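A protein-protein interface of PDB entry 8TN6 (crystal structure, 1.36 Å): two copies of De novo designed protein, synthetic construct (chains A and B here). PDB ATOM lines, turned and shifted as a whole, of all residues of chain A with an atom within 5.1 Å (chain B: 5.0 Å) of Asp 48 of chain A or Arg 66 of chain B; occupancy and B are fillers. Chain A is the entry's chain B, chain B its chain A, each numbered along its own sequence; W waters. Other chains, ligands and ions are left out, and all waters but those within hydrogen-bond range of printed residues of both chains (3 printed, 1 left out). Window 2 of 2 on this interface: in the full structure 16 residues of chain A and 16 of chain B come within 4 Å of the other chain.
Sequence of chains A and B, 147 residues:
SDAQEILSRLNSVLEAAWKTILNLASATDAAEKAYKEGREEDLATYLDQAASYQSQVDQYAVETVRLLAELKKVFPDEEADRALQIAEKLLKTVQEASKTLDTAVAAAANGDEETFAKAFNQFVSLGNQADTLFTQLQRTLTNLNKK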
ATOM      1  N   LEU A  43     -26.635 -28.241   6.588  1.00  0.00           N
ATOM      2  CA  LEU A  43     -27.756 -29.054   6.130  1.00  0.00           C
ATOM      3  C   LEU A  43     -27.911 -28.950   4.618  1.00  0.00           C
ATOM      4  O   LEU A  43     -28.084 -29.955   3.932  1.00  0.00           O
ATOM      5  CB  LEU A  43     -29.030 -28.596   6.840  1.00  0.00           C
ATOM      6  CG  LEU A  43     -30.310 -29.227   6.309  1.00  0.00           C
ATOM      7  CD1 LEU A  43     -30.347 -30.739   6.381  1.00  0.00           C
ATOM      8  CD2 LEU A  43     -31.509 -28.653   7.074  1.00  0.00           C
ATOM      9  N   ALA A  44     -27.854 -27.741   4.083  1.00  0.00           N
ATOM     10  CA  ALA A  44     -27.980 -27.566   2.633  1.00  0.00           C
ATOM     11  C   ALA A  44     -26.929 -28.359   1.885  1.00  0.00           C
ATOM     12  O   ALA A  44     -27.225 -29.011   0.874  1.00  0.00           O
ATOM     13  CB  ALA A  44     -27.848 -26.092   2.267  1.00  0.00           C
ATOM     14  N   THR A  45     -25.689 -28.333   2.358  1.00  0.00           N
ATOM     15  CA  THR A  45     -24.620 -29.073   1.705  1.00  0.00           C
ATOM     16  C   THR A  45     -24.881 -30.568   1.751  1.00  0.00           C
ATOM     17  O   THR A  45     -24.692 -31.287   0.759  1.00  0.00           O
ATOM     18  CB  THR A  45     -23.279 -28.745   2.373  1.00  0.00           C
ATOM     19  OG1 THR A  45     -23.005 -27.354   2.181  1.00  0.00           O
ATOM     20  CG2 THR A  45     -22.142 -29.607   1.818  1.00  0.00           C
ATOM     21  N   TYR A  46     -25.304 -31.091   2.906  1.00  0.00           N
ATOM     22  CA  TYR A  46     -25.544 -32.517   2.991  1.00  0.00           C
ATOM     23  C   TYR A  46     -26.739 -32.930   2.139  1.00  0.00           C
ATOM     24  O   TYR A  46     -26.736 -34.010   1.558  1.00  0.00           O
ATOM     25  CB  TYR A  46     -25.743 -32.956   4.439  1.00  0.00           C
ATOM     26  CG  TYR A  46     -24.473 -32.945   5.242  1.00  0.00           C
ATOM     27  CD1 TYR A  46     -23.341 -33.625   4.815  1.00  0.00           C
ATOM     28  CD2 TYR A  46     -24.412 -32.263   6.446  1.00  0.00           C
ATOM     29  CE1 TYR A  46     -22.172 -33.632   5.558  1.00  0.00           C
ATOM     30  CE2 TYR A  46     -23.238 -32.271   7.216  1.00  0.00           C
ATOM     31  CZ  TYR A  46     -22.139 -32.951   6.749  1.00  0.00           C
ATOM     32  OH  TYR A  46     -20.978 -32.991   7.520  1.00  0.00           O
ATOM     33  N   LEU A  47     -27.761 -32.091   2.054  1.00  0.00           N
ATOM     34  CA  LEU A  47     -28.880 -32.418   1.175  1.00  0.00           C
ATOM     35  C   LEU A  47     -28.444 -32.453  -0.281  1.00  0.00           C
ATOM     36  O   LEU A  47     -28.883 -33.327  -1.040  1.00  0.00           O
ATOM     37  CB  LEU A  47     -30.018 -31.426   1.376  1.00  0.00           C
ATOM     38  CG  LEU A  47     -30.736 -31.527   2.720  1.00  0.00           C
ATOM     39  CD1 LEU A  47     -31.700 -30.369   2.840  1.00  0.00           C
ATOM     40  CD2 LEU A  47     -31.492 -32.804   2.905  1.00  0.00           C
ATOM     41  N   ASP A  48     -27.575 -31.531  -0.692  1.00  0.00           N
ATOM     42  CA  ASP A  48     -27.092 -31.568  -2.071  1.00  0.00           C
ATOM     43  C   ASP A  48     -26.282 -32.830  -2.324  1.00  0.00           C
ATOM     44  O   ASP A  48     -26.400 -33.465  -3.382  1.00  0.00           O
ATOM     45  CB  ASP A  48     -26.252 -30.333  -2.340  1.00  0.00           C
ATOM     46  CG  ASP A  48     -27.085 -29.083  -2.477  1.00  0.00           C
ATOM     47  OD1 ASP A  48     -28.341 -29.185  -2.406  1.00  0.00           O
ATOM     48  OD2 ASP A  48     -26.488 -28.012  -2.643  1.00  0.00           O
ATOM     49  N   GLN A  49     -25.477 -33.262  -1.343  1.00  0.00           N
ATOM     50  CA  GLN A  49     -24.726 -34.489  -1.509  1.00  0.00           C
ATOM     51  C   GLN A  49     -25.672 -35.664  -1.625  1.00  0.00           C
ATOM     52  O   GLN A  49     -25.481 -36.564  -2.454  1.00  0.00           O
ATOM     53  CB  GLN A  49     -23.789 -34.712  -0.318  1.00  0.00           C
ATOM     54  CG  GLN A  49     -22.639 -35.656  -0.580  1.00  0.00           C
ATOM     55  CD  GLN A  49     -21.885 -35.352  -1.868  1.00  0.00           C
ATOM     56  OE1 GLN A  49     -21.212 -34.337  -1.968  1.00  0.00           O
ATOM     57  NE2 GLN A  49     -22.044 -36.222  -2.876  1.00  0.00           N
ATOM     58  N   ALA A  50     -26.682 -35.702  -0.763  1.00  0.00           N
ATOM     59  CA  ALA A  50     -27.661 -36.775  -0.845  1.00  0.00           C
ATOM     60  C   ALA A  50     -28.337 -36.793  -2.207  1.00  0.00           C
ATOM     61  O   ALA A  50     -28.548 -37.860  -2.777  1.00  0.00           O
ATOM     62  CB  ALA A  50     -28.690 -36.628   0.291  1.00  0.00           C
ATOM     63  N   ALA A  51     -28.703 -35.616  -2.725  1.00  0.00           N
ATOM     64  CA  ALA A  51     -29.365 -35.569  -4.025  1.00  0.00           C
ATOM     65  C   ALA A  51     -28.472 -36.121  -5.114  1.00  0.00           C
ATOM     66  O   ALA A  51     -28.957 -36.829  -6.010  1.00  0.00           O
ATOM     67  CB  ALA A  51     -29.826 -34.156  -4.357  1.00  0.00           C
ATOM     68  N   SER A  52     -27.169 -35.868  -5.036  1.00  0.00           N
ATOM     69  CA  SER A  52     -26.264 -36.388  -6.046  1.00  0.00           C
ATOM     70  C   SER A  52     -26.176 -37.908  -5.950  1.00  0.00           C
ATOM     71  O   SER A  52     -26.244 -38.620  -6.965  1.00  0.00           O
ATOM     72  CB  SER A  52     -24.906 -35.725  -5.903  1.00  0.00           C
ATOM     73  OG  SER A  52     -24.004 -36.326  -6.820  1.00  0.00           O
ATOM     74  N   VAL A 105     -35.459 -30.864  -0.203  1.00  0.00           N
ATOM     75  CA  VAL A 105     -34.448 -29.888  -0.593  1.00  0.00           C
ATOM     76  C   VAL A 105     -35.083 -28.535  -0.867  1.00  0.00           C
ATOM     77  O   VAL A 105     -34.557 -27.491  -0.447  1.00  0.00           O
ATOM     78  CB  VAL A 105     -33.650 -30.406  -1.818  1.00  0.00           C
ATOM     79  CG1 VAL A 105     -32.790 -29.321  -2.369  1.00  0.00           C
ATOM     80  CG2 VAL A 105     -32.854 -31.611  -1.473  1.00  0.00           C
ATOM     81  N   ALA A 109     -34.565 -25.037   1.268  1.00  0.00           N
ATOM     82  CA  ALA A 109     -34.109 -23.839   0.568  1.00  0.00           C
ATOM     83  C   ALA A 109     -35.099 -22.699   0.728  1.00  0.00           C
ATOM     84  O   ALA A 109     -34.702 -21.524   0.742  1.00  0.00           O
ATOM     85  CB  ALA A 109     -33.930 -24.148  -0.919  1.00  0.00           C
ATOM     86  N   GLN B  59     -30.012 -29.146  -9.430  1.00  0.00           N
ATOM     87  CA  GLN B  59     -29.048 -28.619  -8.468  1.00  0.00           C
ATOM     88  C   GLN B  59     -28.816 -27.140  -8.697  1.00  0.00           C
ATOM     89  O   GLN B  59     -28.780 -26.360  -7.729  1.00  0.00           O
ATOM     90  CB  GLN B  59     -27.753 -29.432  -8.553  1.00  0.00           C
ATOM     91  CG  GLN B  59     -26.575 -28.880  -7.753  1.00  0.00           C
ATOM     92  CD  GLN B  59     -26.779 -28.965  -6.266  1.00  0.00           C
ATOM     93  OE1 GLN B  59     -27.375 -29.914  -5.761  1.00  0.00           O
ATOM     94  NE2 GLN B  59     -26.299 -27.954  -5.551  1.00  0.00           N
ATOM     95  N   VAL B  62     -31.755 -25.204  -7.306  1.00  0.00           N
ATOM     96  CA  VAL B  62     -31.656 -25.111  -5.850  1.00  0.00           C
ATOM     97  C   VAL B  62     -30.653 -24.031  -5.466  1.00  0.00           C
ATOM     98  O   VAL B  62     -30.915 -23.201  -4.578  1.00  0.00           O
ATOM     99  CB  VAL B  62     -31.252 -26.484  -5.276  1.00  0.00           C
ATOM    100  CG1 VAL B  62     -31.098 -26.390  -3.762  1.00  0.00           C
ATOM    101  CG2 VAL B  62     -32.294 -27.542  -5.580  1.00  0.00           C
ATOM    102  N   GLU B  63     -29.497 -24.033  -6.091  1.00  0.00           N
ATOM    103  CA  GLU B  63     -28.487 -23.038  -5.776  1.00  0.00           C
ATOM    104  C   GLU B  63     -29.020 -21.646  -6.030  1.00  0.00           C
ATOM    105  O   GLU B  63     -28.732 -20.714  -5.268  1.00  0.00           O
ATOM    106  CB  GLU B  63     -27.229 -23.253  -6.592  1.00  0.00           C
ATOM    107  CG  GLU B  63     -26.394 -24.429  -6.150  1.00  0.00           C
ATOM    108  CD  GLU B  63     -25.306 -24.763  -7.153  1.00  0.00           C
ATOM    109  OE1 GLU B  63     -24.823 -23.819  -7.826  1.00  0.00           O
ATOM    110  OE2 GLU B  63     -24.889 -25.938  -7.222  1.00  0.00           O
ATOM    111  N   THR B  64     -29.786 -21.469  -7.100  1.00  0.00           N
ATOM    112  CA  THR B  64     -30.339 -20.168  -7.451  1.00  0.00           C
ATOM    113  C   THR B  64     -31.291 -19.682  -6.375  1.00  0.00           C
ATOM    114  O   THR B  64     -31.221 -18.520  -5.935  1.00  0.00           O
ATOM    115  CB  THR B  64     -31.040 -20.302  -8.806  1.00  0.00           C
ATOM    116  OG1 THR B  64     -30.060 -20.598  -9.810  1.00  0.00           O
ATOM    117  CG2 THR B  64     -31.781 -19.047  -9.207  1.00  0.00           C
ATOM    118  N   VAL B  65     -32.165 -20.564  -5.909  1.00  0.00           N
ATOM    119  CA  VAL B  65     -33.051 -20.203  -4.816  1.00  0.00           C
ATOM    120  C   VAL B  65     -32.237 -19.819  -3.590  1.00  0.00           C
ATOM    121  O   VAL B  65     -32.520 -18.812  -2.937  1.00  0.00           O
ATOM    122  CB  VAL B  65     -34.030 -21.339  -4.490  1.00  0.00           C
ATOM    123  CG1 VAL B  65     -34.721 -21.091  -3.148  1.00  0.00           C
ATOM    124  CG2 VAL B  65     -35.056 -21.487  -5.594  1.00  0.00           C
ATOM    125  N   ARG B  66     -31.241 -20.621  -3.240  1.00  0.00           N
ATOM    126  CA  ARG B  66     -30.489 -20.326  -2.022  1.00  0.00           C
ATOM    127  C   ARG B  66     -29.783 -18.984  -2.117  1.00  0.00           C
ATOM    128  O   ARG B  66     -29.759 -18.225  -1.138  1.00  0.00           O
ATOM    129  CB  ARG B  66     -29.500 -21.444  -1.760  1.00  0.00           C
ATOM    130  CG  ARG B  66     -30.182 -22.688  -1.248  1.00  0.00           C
ATOM    131  CD  ARG B  66     -29.108 -23.719  -1.029  1.00  0.00           C
ATOM    132  NE  ARG B  66     -29.622 -25.057  -0.781  1.00  0.00           N
ATOM    133  CZ  ARG B  66     -28.971 -26.159  -1.139  1.00  0.00           C
ATOM    134  NH1 ARG B  66     -27.836 -26.092  -1.814  1.00  0.00           N
ATOM    135  NH2 ARG B  66     -29.462 -27.355  -0.797  1.00  0.00           N
ATOM    136  N   LEU B  67     -29.191 -18.666  -3.265  1.00  0.00           N
ATOM    137  CA  LEU B  67     -28.548 -17.367  -3.430  1.00  0.00           C
ATOM    138  C   LEU B  67     -29.549 -16.235  -3.312  1.00  0.00           C
ATOM    139  O   LEU B  67     -29.276 -15.226  -2.643  1.00  0.00           O
ATOM    140  CB  LEU B  67     -27.858 -17.292  -4.787  1.00  0.00           C
ATOM    141  CG  LEU B  67     -26.586 -18.120  -4.859  1.00  0.00           C
ATOM    142  CD1 LEU B  67     -26.213 -18.468  -6.295  1.00  0.00           C
ATOM    143  CD2 LEU B  67     -25.426 -17.428  -4.172  1.00  0.00           C
ATOM    144  N   LEU B  68     -30.708 -16.358  -3.948  1.00  0.00           N
ATOM    145  CA  LEU B  68     -31.679 -15.276  -3.869  1.00  0.00           C
ATOM    146  C   LEU B  68     -32.304 -15.190  -2.484  1.00  0.00           C
ATOM    147  O   LEU B  68     -32.662 -14.092  -2.029  1.00  0.00           O
ATOM    148  CB  LEU B  68     -32.746 -15.420  -4.959  1.00  0.00           C
ATOM    149  CG  LEU B  68     -32.186 -15.065  -6.330  1.00  0.00           C
ATOM    150  CD1 LEU B  68     -33.069 -15.600  -7.462  1.00  0.00           C
ATOM    151  CD2 LEU B  68     -32.039 -13.540  -6.487  1.00  0.00           C
ATOM    152  N   ALA B  69     -32.413 -16.315  -1.781  1.00  0.00           N
ATOM    153  CA  ALA B  69     -32.859 -16.244  -0.396  1.00  0.00           C
ATOM    154  C   ALA B  69     -31.849 -15.476   0.439  1.00  0.00           C
ATOM    155  O   ALA B  69     -32.234 -14.650   1.283  1.00  0.00           O
ATOM    156  CB  ALA B  69     -33.065 -17.645   0.158  1.00  0.00           C
ATOM    157  N   GLU B  70     -30.559 -15.701   0.206  1.00  0.00           N
ATOM    158  CA  GLU B  70     -29.537 -14.927   0.897  1.00  0.00           C
ATOM    159  C   GLU B  70     -29.678 -13.455   0.566  1.00  0.00           C
ATOM    160  O   GLU B  70     -29.625 -12.601   1.459  1.00  0.00           O
ATOM    161  CB  GLU B  70     -28.138 -15.378   0.478  1.00  0.00           C
ATOM    162  CG  GLU B  70     -27.712 -16.765   0.902  1.00  0.00           C
ATOM    163  CD  GLU B  70     -26.347 -17.142   0.333  1.00  0.00           C
ATOM    164  OE1 GLU B  70     -25.499 -16.236   0.148  1.00  0.00           O
ATOM    165  OE2 GLU B  70     -26.121 -18.348   0.086  1.00  0.00           O
HETATM  166  O   HOH W   1     -29.720 -30.264  -4.530  1.00  0.00           O
HETATM  167  O   HOH W   2     -26.597 -32.294  -5.849  1.00  0.00           O
HETATM  168  O   HOH W   3     -31.879 -27.100   0.428  1.00  0.00           O
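NH2 of Arg 66 of chain B lies within hydrogen-bond range of O of Ala 44 of chain A (3.2 Å). The side-chain carboxylate (OD2) of Asp 48 of chain A lies within hydrogen-bond range of the side-chain amide nitrogen (NE2) of Gln 59 of chain B, 2.9 Å away. The guanidinium group (NH1) of Arg 66 of chain B is in salt-bridge range of the side-chain carboxylate (OD2) of Asp 48 of chain A (2.5 Å).
The side-chain amide nitrogen of Gln 59 of chain B lies within hydrogen-bond range of the side-chain carboxylate of Glu 63 of chain B (3.0 Å).
Among the printed residues, merely in contact across the chains: Val 105 of chain A with Val 62 of chain B (3.7 Å) and Ala 109 of chain A with Val 65 of chain B (3.9 Å).
Of chain A, only Ala 44 (3.2 Å) and Asp 48 (2.5 Å) come within 4 Å of Arg 66 of chain B. Printed residues of chain B within 4 Å of Ala 109 of chain A: Val 65 (3.9 Å). Of the printed residues of chain A, Val 65 of chain B touches Ala 109 (3.9 Å). Printed residues of chain B within 4 Å of Val 105 of chain A: Val 62. Printed residues of chain A within 4 Å of Gln 59 of chain B: Asp 48. Of the printed residues of chain A, Val 62 of chain B touches Val 105. Leu 67 of chain B touches none of the printed residues of chain A.
Along chain B the printed residues that touch a printed residue of chain A span positions 59 to 66. Hydrophobic or aromatic side chains of chain A within 4 Å of the printed part of chain B: Ala 44, Val 105 and Ala 109. Among the printed residues, 5 pairs touch across the chains.
No position is printed for both chains. Of the 5 pairs that touch across the chains among the printed residues, none has its exchanged pair printed and touching as well.
Water W2 bridges the side-chain amide oxygen (OE1) of Gln 59 of chain B (2.5 Å) and the backbone carbonyl oxygen (O) of Asp 48 of chain A (2.7 Å). Water W1 bridges the side-chain amide oxygen of Gln 59 of chain B (2.7 Å) and the side-chain carboxylate of Asp 48 of chain A (2.8 Å). Water W3 lies within hydrogen-bond range of NH2 of Arg 66 of chain B (2.7 Å), O of Val 105 of chain A (2.8 Å) and N of Ala 109 of chain A (3.5 Å).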
